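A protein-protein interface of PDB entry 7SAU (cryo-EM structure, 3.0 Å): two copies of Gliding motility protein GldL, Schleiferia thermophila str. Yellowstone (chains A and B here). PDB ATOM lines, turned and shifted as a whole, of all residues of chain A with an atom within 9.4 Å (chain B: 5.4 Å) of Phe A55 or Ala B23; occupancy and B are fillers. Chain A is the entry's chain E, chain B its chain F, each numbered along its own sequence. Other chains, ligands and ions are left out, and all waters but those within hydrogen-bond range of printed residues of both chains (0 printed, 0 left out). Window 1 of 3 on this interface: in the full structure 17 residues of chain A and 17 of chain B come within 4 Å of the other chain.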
ATOM      1  N   ASN A   7      21.528   2.946  -7.707  1.00  0.00           N
ATOM      2  CA  ASN A   7      22.033   1.659  -7.249  1.00  0.00           C
ATOM      3  C   ASN A   7      21.769   0.580  -8.289  1.00  0.00           C
ATOM      4  O   ASN A   7      21.248  -0.493  -7.966  1.00  0.00           O
ATOM      5  CB  ASN A   7      21.405   1.274  -5.908  1.00  0.00           C
ATOM      6  CG  ASN A   7      21.948   2.092  -4.754  1.00  0.00           C
ATOM      7  OD1 ASN A   7      22.127   3.303  -4.867  1.00  0.00           O
ATOM      8  ND2 ASN A   7      22.217   1.432  -3.636  1.00  0.00           N
ATOM      9  N   LEU A  15      30.413  -1.658  -5.236  1.00  0.00           N
ATOM     10  CA  LEU A  15      30.055  -2.025  -3.873  1.00  0.00           C
ATOM     11  C   LEU A  15      30.564  -3.416  -3.525  1.00  0.00           C
ATOM     12  O   LEU A  15      30.896  -3.683  -2.366  1.00  0.00           O
ATOM     13  CB  LEU A  15      28.538  -1.953  -3.709  1.00  0.00           C
ATOM     14  CG  LEU A  15      27.919  -2.194  -2.340  1.00  0.00           C
ATOM     15  CD1 LEU A  15      28.380  -1.113  -1.395  1.00  0.00           C
ATOM     16  CD2 LEU A  15      26.410  -2.209  -2.439  1.00  0.00           C
ATOM     17  N   LEU A  18      34.098  -3.217  -2.393  1.00  0.00           N
ATOM     18  CA  LEU A  18      34.185  -2.598  -1.079  1.00  0.00           C
ATOM     19  C   LEU A  18      33.743  -3.564   0.014  1.00  0.00           C
ATOM     20  O   LEU A  18      34.156  -3.424   1.169  1.00  0.00           O
ATOM     21  CB  LEU A  18      33.345  -1.323  -1.064  1.00  0.00           C
ATOM     22  CG  LEU A  18      33.470  -0.372   0.117  1.00  0.00           C
ATOM     23  CD1 LEU A  18      34.871   0.190   0.150  1.00  0.00           C
ATOM     24  CD2 LEU A  18      32.456   0.745  -0.006  1.00  0.00           C
ATOM     25  N   TYR A  19      32.909  -4.547  -0.335  1.00  0.00           N
ATOM     26  CA  TYR A  19      32.547  -5.598   0.613  1.00  0.00           C
ATOM     27  C   TYR A  19      33.756  -6.437   0.997  1.00  0.00           C
ATOM     28  O   TYR A  19      33.944  -6.765   2.173  1.00  0.00           O
ATOM     29  CB  TYR A  19      31.470  -6.498   0.012  1.00  0.00           C
ATOM     30  CG  TYR A  19      30.055  -6.149   0.390  1.00  0.00           C
ATOM     31  CD1 TYR A  19      29.564  -6.438   1.650  1.00  0.00           C
ATOM     32  CD2 TYR A  19      29.203  -5.547  -0.522  1.00  0.00           C
ATOM     33  CE1 TYR A  19      28.268  -6.132   1.994  1.00  0.00           C
ATOM     34  CE2 TYR A  19      27.909  -5.234  -0.187  1.00  0.00           C
ATOM     35  CZ  TYR A  19      27.445  -5.528   1.072  1.00  0.00           C
ATOM     36  OH  TYR A  19      26.151  -5.218   1.412  1.00  0.00           O
ATOM     37  N   GLY A  47      38.694  -0.394   8.405  1.00  0.00           N
ATOM     38  CA  GLY A  47      37.818  -1.525   8.154  1.00  0.00           C
ATOM     39  C   GLY A  47      36.413  -1.325   8.687  1.00  0.00           C
ATOM     40  O   GLY A  47      35.434  -1.659   8.016  1.00  0.00           O
ATOM     41  N   LEU A  48      36.289  -0.794   9.902  1.00  0.00           N
ATOM     42  CA  LEU A  48      34.967  -0.630  10.494  1.00  0.00           C
ATOM     43  C   LEU A  48      34.221   0.543   9.873  1.00  0.00           C
ATOM     44  O   LEU A  48      33.004   0.472   9.677  1.00  0.00           O
ATOM     45  CB  LEU A  48      35.083  -0.456  12.007  1.00  0.00           C
ATOM     46  CG  LEU A  48      35.376  -1.725  12.804  1.00  0.00           C
ATOM     47  CD1 LEU A  48      35.509  -1.408  14.275  1.00  0.00           C
ATOM     48  CD2 LEU A  48      34.300  -2.765  12.576  1.00  0.00           C
ATOM     49  N   SER A  49      34.925   1.632   9.561  1.00  0.00           N
ATOM     50  CA  SER A  49      34.265   2.758   8.910  1.00  0.00           C
ATOM     51  C   SER A  49      33.835   2.407   7.494  1.00  0.00           C
ATOM     52  O   SER A  49      32.800   2.889   7.024  1.00  0.00           O
ATOM     53  CB  SER A  49      35.179   3.979   8.897  1.00  0.00           C
ATOM     54  OG  SER A  49      34.674   4.979   8.035  1.00  0.00           O
ATOM     55  N   THR A  50      34.620   1.587   6.795  1.00  0.00           N
ATOM     56  CA  THR A  50      34.176   1.064   5.509  1.00  0.00           C
ATOM     57  C   THR A  50      32.932   0.208   5.675  1.00  0.00           C
ATOM     58  O   THR A  50      31.982   0.315   4.893  1.00  0.00           O
ATOM     59  CB  THR A  50      35.292   0.249   4.861  1.00  0.00           C
ATOM     60  OG1 THR A  50      36.369   1.118   4.493  1.00  0.00           O
ATOM     61  CG2 THR A  50      34.782  -0.471   3.639  1.00  0.00           C
ATOM     62  N   GLU A  51      32.919  -0.639   6.699  1.00  0.00           N
ATOM     63  CA  GLU A  51      31.773  -1.507   6.935  1.00  0.00           C
ATOM     64  C   GLU A  51      30.555  -0.714   7.387  1.00  0.00           C
ATOM     65  O   GLU A  51      29.418  -1.089   7.083  1.00  0.00           O
ATOM     66  CB  GLU A  51      32.142  -2.564   7.965  1.00  0.00           C
ATOM     67  CG  GLU A  51      31.123  -3.638   8.094  1.00  0.00           C
ATOM     68  CD  GLU A  51      31.452  -4.605   9.187  1.00  0.00           C
ATOM     69  OE1 GLU A  51      30.529  -5.308   9.632  1.00  0.00           O
ATOM     70  OE2 GLU A  51      32.630  -4.660   9.593  1.00  0.00           O
ATOM     71  N   ALA A  52      30.767   0.373   8.128  1.00  0.00           N
ATOM     72  CA  ALA A  52      29.654   1.241   8.492  1.00  0.00           C
ATOM     73  C   ALA A  52      29.055   1.906   7.262  1.00  0.00           C
ATOM     74  O   ALA A  52      27.836   2.078   7.171  1.00  0.00           O
ATOM     75  CB  ALA A  52      30.113   2.291   9.501  1.00  0.00           C
ATOM     76  N   VAL A  53      29.901   2.291   6.305  1.00  0.00           N
ATOM     77  CA  VAL A  53      29.409   2.870   5.059  1.00  0.00           C
ATOM     78  C   VAL A  53      28.646   1.827   4.252  1.00  0.00           C
ATOM     79  O   VAL A  53      27.629   2.134   3.619  1.00  0.00           O
ATOM     80  CB  VAL A  53      30.580   3.472   4.263  1.00  0.00           C
ATOM     81  CG1 VAL A  53      30.219   3.633   2.803  1.00  0.00           C
ATOM     82  CG2 VAL A  53      30.985   4.802   4.859  1.00  0.00           C
ATOM     83  N   ILE A  54      29.118   0.580   4.269  1.00  0.00           N
ATOM     84  CA  ILE A  54      28.436  -0.497   3.557  1.00  0.00           C
ATOM     85  C   ILE A  54      27.013  -0.658   4.075  1.00  0.00           C
ATOM     86  O   ILE A  54      26.051  -0.719   3.301  1.00  0.00           O
ATOM     87  CB  ILE A  54      29.220  -1.811   3.702  1.00  0.00           C
ATOM     88  CG1 ILE A  54      30.525  -1.762   2.911  1.00  0.00           C
ATOM     89  CG2 ILE A  54      28.368  -2.971   3.257  1.00  0.00           C
ATOM     90  CD1 ILE A  54      30.335  -1.799   1.438  1.00  0.00           C
ATOM     91  N   PHE A  55      26.863  -0.733   5.397  1.00  0.00           N
ATOM     92  CA  PHE A  55      25.548  -0.908   6.001  1.00  0.00           C
ATOM     93  C   PHE A  55      24.637   0.270   5.692  1.00  0.00           C
ATOM     94  O   PHE A  55      23.433   0.093   5.480  1.00  0.00           O
ATOM     95  CB  PHE A  55      25.694  -1.081   7.508  1.00  0.00           C
ATOM     96  CG  PHE A  55      25.822  -2.500   7.937  1.00  0.00           C
ATOM     97  CD1 PHE A  55      24.828  -3.410   7.659  1.00  0.00           C
ATOM     98  CD2 PHE A  55      26.946  -2.932   8.605  1.00  0.00           C
ATOM     99  CE1 PHE A  55      24.946  -4.716   8.057  1.00  0.00           C
ATOM    100  CE2 PHE A  55      27.066  -4.241   8.998  1.00  0.00           C
ATOM    101  CZ  PHE A  55      26.068  -5.130   8.720  1.00  0.00           C
ATOM    102  N   PHE A  56      25.193   1.481   5.678  1.00  0.00           N
ATOM    103  CA  PHE A  56      24.399   2.664   5.376  1.00  0.00           C
ATOM    104  C   PHE A  56      23.813   2.593   3.972  1.00  0.00           C
ATOM    105  O   PHE A  56      22.648   2.943   3.761  1.00  0.00           O
ATOM    106  CB  PHE A  56      25.256   3.917   5.547  1.00  0.00           C
ATOM    107  CG  PHE A  56      24.547   5.193   5.212  1.00  0.00           C
ATOM    108  CD1 PHE A  56      23.801   5.855   6.165  1.00  0.00           C
ATOM    109  CD2 PHE A  56      24.644   5.743   3.946  1.00  0.00           C
ATOM    110  CE1 PHE A  56      23.157   7.034   5.860  1.00  0.00           C
ATOM    111  CE2 PHE A  56      23.999   6.918   3.636  1.00  0.00           C
ATOM    112  CZ  PHE A  56      23.255   7.565   4.594  1.00  0.00           C
ATOM    113  N   PHE A  57      24.602   2.138   2.999  1.00  0.00           N
ATOM    114  CA  PHE A  57      24.105   2.045   1.632  1.00  0.00           C
ATOM    115  C   PHE A  57      23.138   0.887   1.439  1.00  0.00           C
ATOM    116  O   PHE A  57      22.358   0.904   0.483  1.00  0.00           O
ATOM    117  CB  PHE A  57      25.271   1.915   0.655  1.00  0.00           C
ATOM    118  CG  PHE A  57      25.969   3.209   0.380  1.00  0.00           C
ATOM    119  CD1 PHE A  57      25.249   4.340   0.051  1.00  0.00           C
ATOM    120  CD2 PHE A  57      27.346   3.298   0.454  1.00  0.00           C
ATOM    121  CE1 PHE A  57      25.887   5.534  -0.202  1.00  0.00           C
ATOM    122  CE2 PHE A  57      27.987   4.490   0.202  1.00  0.00           C
ATOM    123  CZ  PHE A  57      27.257   5.609  -0.125  1.00  0.00           C
ATOM    124  N   SER A  58      23.168  -0.116   2.315  1.00  0.00           N
ATOM    125  CA  SER A  58      22.202  -1.203   2.228  1.00  0.00           C
ATOM    126  C   SER A  58      20.817  -0.789   2.697  1.00  0.00           C
ATOM    127  O   SER A  58      19.862  -1.544   2.492  1.00  0.00           O
ATOM    128  CB  SER A  58      22.684  -2.406   3.036  1.00  0.00           C
ATOM    129  OG  SER A  58      23.879  -2.930   2.488  1.00  0.00           O
ATOM    130  N   ALA A  59      20.687   0.377   3.326  1.00  0.00           N
ATOM    131  CA  ALA A  59      19.365   0.872   3.688  1.00  0.00           C
ATOM    132  C   ALA A  59      18.557   1.226   2.449  1.00  0.00           C
ATOM    133  O   ALA A  59      17.341   1.010   2.411  1.00  0.00           O
ATOM    134  CB  ALA A  59      19.494   2.081   4.610  1.00  0.00           C
ATOM    135  N   PHE A  60      19.211   1.765   1.426  1.00  0.00           N
ATOM    136  CA  PHE A  60      18.538   2.236   0.226  1.00  0.00           C
ATOM    137  C   PHE A  60      18.424   1.174  -0.856  1.00  0.00           C
ATOM    138  O   PHE A  60      17.921   1.471  -1.944  1.00  0.00           O
ATOM    139  CB  PHE A  60      19.267   3.459  -0.331  1.00  0.00           C
ATOM    140  CG  PHE A  60      19.489   4.536   0.684  1.00  0.00           C
ATOM    141  CD1 PHE A  60      18.421   5.223   1.226  1.00  0.00           C
ATOM    142  CD2 PHE A  60      20.764   4.857   1.105  1.00  0.00           C
ATOM    143  CE1 PHE A  60      18.622   6.211   2.161  1.00  0.00           C
ATOM    144  CE2 PHE A  60      20.969   5.844   2.041  1.00  0.00           C
ATOM    145  CZ  PHE A  60      19.897   6.522   2.569  1.00  0.00           C
ATOM    146  N   GLU A  61      18.876  -0.048  -0.593  1.00  0.00           N
ATOM    147  CA  GLU A  61      18.768  -1.113  -1.580  1.00  0.00           C
ATOM    148  C   GLU A  61      17.319  -1.567  -1.705  1.00  0.00           C
ATOM    149  O   GLU A  61      16.638  -1.790  -0.699  1.00  0.00           O
ATOM    150  CB  GLU A  61      19.664  -2.285  -1.190  1.00  0.00           C
ATOM    151  CG  GLU A  61      19.188  -3.632  -1.695  1.00  0.00           C
ATOM    152  CD  GLU A  61      20.180  -4.741  -1.413  1.00  0.00           C
ATOM    153  OE1 GLU A  61      21.213  -4.465  -0.769  1.00  0.00           O
ATOM    154  OE2 GLU A  61      19.925  -5.889  -1.833  1.00  0.00           O
ATOM    155  N   LEU B  18      15.489   1.194   8.397  1.00  0.00           N
ATOM    156  CA  LEU B  18      15.875   1.309   9.798  1.00  0.00           C
ATOM    157  C   LEU B  18      16.927   0.281  10.180  1.00  0.00           C
ATOM    158  O   LEU B  18      17.754   0.542  11.059  1.00  0.00           O
ATOM    159  CB  LEU B  18      14.647   1.167  10.694  1.00  0.00           C
ATOM    160  CG  LEU B  18      14.776   1.773  12.088  1.00  0.00           C
ATOM    161  CD1 LEU B  18      15.000   3.267  11.989  1.00  0.00           C
ATOM    162  CD2 LEU B  18      13.546   1.468  12.921  1.00  0.00           C
ATOM    163  N   TYR B  19      16.915  -0.892   9.545  1.00  0.00           N
ATOM    164  CA  TYR B  19      17.936  -1.886   9.852  1.00  0.00           C
ATOM    165  C   TYR B  19      19.287  -1.485   9.280  1.00  0.00           C
ATOM    166  O   TYR B  19      20.325  -1.725   9.905  1.00  0.00           O
ATOM    167  CB  TYR B  19      17.530  -3.260   9.327  1.00  0.00           C
ATOM    168  CG  TYR B  19      18.570  -4.308   9.633  1.00  0.00           C
ATOM    169  CD1 TYR B  19      19.449  -4.751   8.656  1.00  0.00           C
ATOM    170  CD2 TYR B  19      18.695  -4.830  10.911  1.00  0.00           C
ATOM    171  CE1 TYR B  19      20.413  -5.696   8.940  1.00  0.00           C
ATOM    172  CE2 TYR B  19      19.653  -5.775  11.204  1.00  0.00           C
ATOM    173  CZ  TYR B  19      20.509  -6.206  10.216  1.00  0.00           C
ATOM    174  OH  TYR B  19      21.464  -7.150  10.507  1.00  0.00           O
ATOM    175  N   GLY B  20      19.297  -0.892   8.088  1.00  0.00           N
ATOM    176  CA  GLY B  20      20.554  -0.446   7.512  1.00  0.00           C
ATOM    177  C   GLY B  20      21.199   0.663   8.318  1.00  0.00           C
ATOM    178  O   GLY B  20      22.408   0.653   8.548  1.00  0.00           O
ATOM    179  N   PHE B  21      20.400   1.634   8.760  1.00  0.00           N
ATOM    180  CA  PHE B  21      20.937   2.698   9.597  1.00  0.00           C
ATOM    181  C   PHE B  21      21.298   2.189  10.983  1.00  0.00           C
ATOM    182  O   PHE B  21      22.241   2.693  11.598  1.00  0.00           O
ATOM    183  CB  PHE B  21      19.932   3.842   9.703  1.00  0.00           C
ATOM    184  CG  PHE B  21      19.625   4.501   8.394  1.00  0.00           C
ATOM    185  CD1 PHE B  21      20.577   4.568   7.396  1.00  0.00           C
ATOM    186  CD2 PHE B  21      18.381   5.056   8.160  1.00  0.00           C
ATOM    187  CE1 PHE B  21      20.296   5.173   6.191  1.00  0.00           C
ATOM    188  CE2 PHE B  21      18.096   5.662   6.957  1.00  0.00           C
ATOM    189  CZ  PHE B  21      19.055   5.722   5.972  1.00  0.00           C
ATOM    190  N   GLY B  22      20.561   1.205  11.492  1.00  0.00           N
ATOM    191  CA  GLY B  22      20.847   0.697  12.822  1.00  0.00           C
ATOM    192  C   GLY B  22      22.185  -0.007  12.912  1.00  0.00           C
ATOM    193  O   GLY B  22      22.944   0.208  13.859  1.00  0.00           O
ATOM    194  N   ALA B  23      22.499  -0.852  11.930  1.00  0.00           N
ATOM    195  CA  ALA B  23      23.747  -1.606  11.984  1.00  0.00           C
ATOM    196  C   ALA B  23      24.954  -0.723  11.700  1.00  0.00           C
ATOM    197  O   ALA B  23      26.065  -1.044  12.133  1.00  0.00           O
ATOM    198  CB  ALA B  23      23.698  -2.774  11.004  1.00  0.00           C
ATOM    199  N   SER B  24      24.765   0.377  10.970  1.00  0.00           N
ATOM    200  CA  SER B  24      25.845   1.343  10.801  1.00  0.00           C
ATOM    201  C   SER B  24      26.206   2.004  12.123  1.00  0.00           C
ATOM    202  O   SER B  24      27.386   2.183  12.434  1.00  0.00           O
ATOM    203  CB  SER B  24      25.451   2.402   9.776  1.00  0.00           C
ATOM    204  OG  SER B  24      25.702   1.959   8.460  1.00  0.00           O
ATOM    205  N   ILE B  25      25.199   2.385  12.910  1.00  0.00           N
ATOM    206  CA  ILE B  25      25.458   3.106  14.150  1.00  0.00           C
ATOM    207  C   ILE B  25      26.087   2.189  15.192  1.00  0.00           C
ATOM    208  O   ILE B  25      26.884   2.639  16.020  1.00  0.00           O
ATOM    209  CB  ILE B  25      24.162   3.758  14.662  1.00  0.00           C
ATOM    210  CG1 ILE B  25      23.603   4.716  13.615  1.00  0.00           C
ATOM    211  CG2 ILE B  25      24.427   4.558  15.905  1.00  0.00           C
ATOM    212  CD1 ILE B  25      24.533   5.848  13.278  1.00  0.00           C
ATOM    213  N   VAL B  26      25.751   0.898  15.175  1.00  0.00           N
ATOM    214  CA  VAL B  26      26.405  -0.046  16.079  1.00  0.00           C
ATOM    215  C   VAL B  26      27.889  -0.152  15.753  1.00  0.00           C
ATOM    216  O   VAL B  26      28.741  -0.131  16.646  1.00  0.00           O
ATOM    217  CB  VAL B  26      25.727  -1.425  16.008  1.00  0.00           C
ATOM    218  CG1 VAL B  26      26.449  -2.408  16.909  1.00  0.00           C
ATOM    219  CG2 VAL B  26      24.285  -1.330  16.400  1.00  0.00           C
ATOM    220  N   ILE B  27      28.219  -0.273  14.469  1.00  0.00           N
ATOM    221  CA  ILE B  27      29.609  -0.460  14.076  1.00  0.00           C
ATOM    222  C   ILE B  27      30.408   0.815  14.292  1.00  0.00           C
ATOM    223  O   ILE B  27      31.547   0.774  14.769  1.00  0.00           O
ATOM    224  CB  ILE B  27      29.681  -0.941  12.621  1.00  0.00           C
ATOM    225  CG1 ILE B  27      29.362  -2.425  12.572  1.00  0.00           C
ATOM    226  CG2 ILE B  27      31.045  -0.679  12.034  1.00  0.00           C
ATOM    227  CD1 ILE B  27      29.238  -2.934  11.203  1.00  0.00           C
ATOM    228  N   LEU B  28      29.833   1.964  13.940  1.00  0.00           N
ATOM    229  CA  LEU B  28      30.483   3.227  14.260  1.00  0.00           C
ATOM    230  C   LEU B  28      30.652   3.381  15.763  1.00  0.00           C
ATOM    231  O   LEU B  28      31.711   3.802  16.237  1.00  0.00           O
ATOM    232  CB  LEU B  28      29.678   4.390  13.691  1.00  0.00           C
ATOM    233  CG  LEU B  28      29.955   4.823  12.255  1.00  0.00           C
ATOM    234  CD1 LEU B  28      29.186   6.089  11.947  1.00  0.00           C
ATOM    235  CD2 LEU B  28      31.434   5.036  12.036  1.00  0.00           C
ATOM    236  N   GLU B  51      18.318  -1.900  16.723  1.00  0.00           N
ATOM    237  CA  GLU B  51      18.317  -3.331  16.443  1.00  0.00           C
ATOM    238  C   GLU B  51      17.340  -4.078  17.336  1.00  0.00           C
ATOM    239  O   GLU B  51      16.817  -5.121  16.935  1.00  0.00           O
ATOM    240  CB  GLU B  51      19.721  -3.903  16.604  1.00  0.00           C
ATOM    241  CG  GLU B  51      20.745  -3.257  15.703  1.00  0.00           C
ATOM    242  CD  GLU B  51      20.835  -3.934  14.356  1.00  0.00           C
ATOM    243  OE1 GLU B  51      20.165  -3.468  13.412  1.00  0.00           O
ATOM    244  OE2 GLU B  51      21.573  -4.933  14.240  1.00  0.00           O
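Among the printed residues, pairs that only touch across the chains: Leu A48 with Ile B27 (3.3 Å), Glu A51 with Ile B27 (3.1 Å), Ala A52 with Leu B28 (3.7 Å), Phe A55 with Ala B23 (3.6 Å), Phe A55 with Ser B24 (3.2 Å), Phe A55 with Ile B27 (3.4 Å), Phe A56 with Phe B21 (3.4 Å), Ala A59 with Gly B20 (3.99 Å), Ala A59 with Phe B21 (3.6 Å) and Phe A60 with Phe B21 (3.6 Å).
O of Ala A52 lies within hydrogen-bond range of OG of Ser B24, 2.5 Å away.
The backbone carbonyl oxygen (O) of Gly B20 sits close to the backbone carbonyl oxygen (O) of Phe A55 (3.3 Å).
OG of Ser B24 sits at hydrogen-bond distance from N of Phe A56, at 2.9 Å.
3 positions are printed for both chains.
Printed residues of chain B that touch a printed residue of chain A: Gly B20, Phe B21, Ala B23, Ser B24, Ile B27 and Leu B28.
Hydrophobic or aromatic side chains of chain B that line the printed part of chain A: Phe B21, Ala B23, Ile B27 and Leu B28.
Among the printed residues, no Asp or Glu carboxylate lies within 4 Å of a Lys or Arg side-chain nitrogen of the other chain.
Ala B23 touches just one residue of chain A: Phe A55.
No residue of chain A comes within 4 Å of Gly B22.
Of chain A, only Ala A52, Phe A55 and Phe A56 come within 4 Å of Ser B24.
No residue of chain A comes within 4 Å of Val B26.
Of the printed residues of chain A, Leu B28 touches Ala A52 (3.7 Å).
Printed residues of chain B within 4 Å of Phe A56: Phe B21 and Ser B24.
Of the printed residues of chain A, Gly B20 touches Phe A55 (3.3 Å) and Ala A59 (3.99 Å).
Glu A61 touches none of the printed residues of chain B.
The nearest residue of chain A that does not touch Ala B23 is Ala A52 (5.6 Å).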
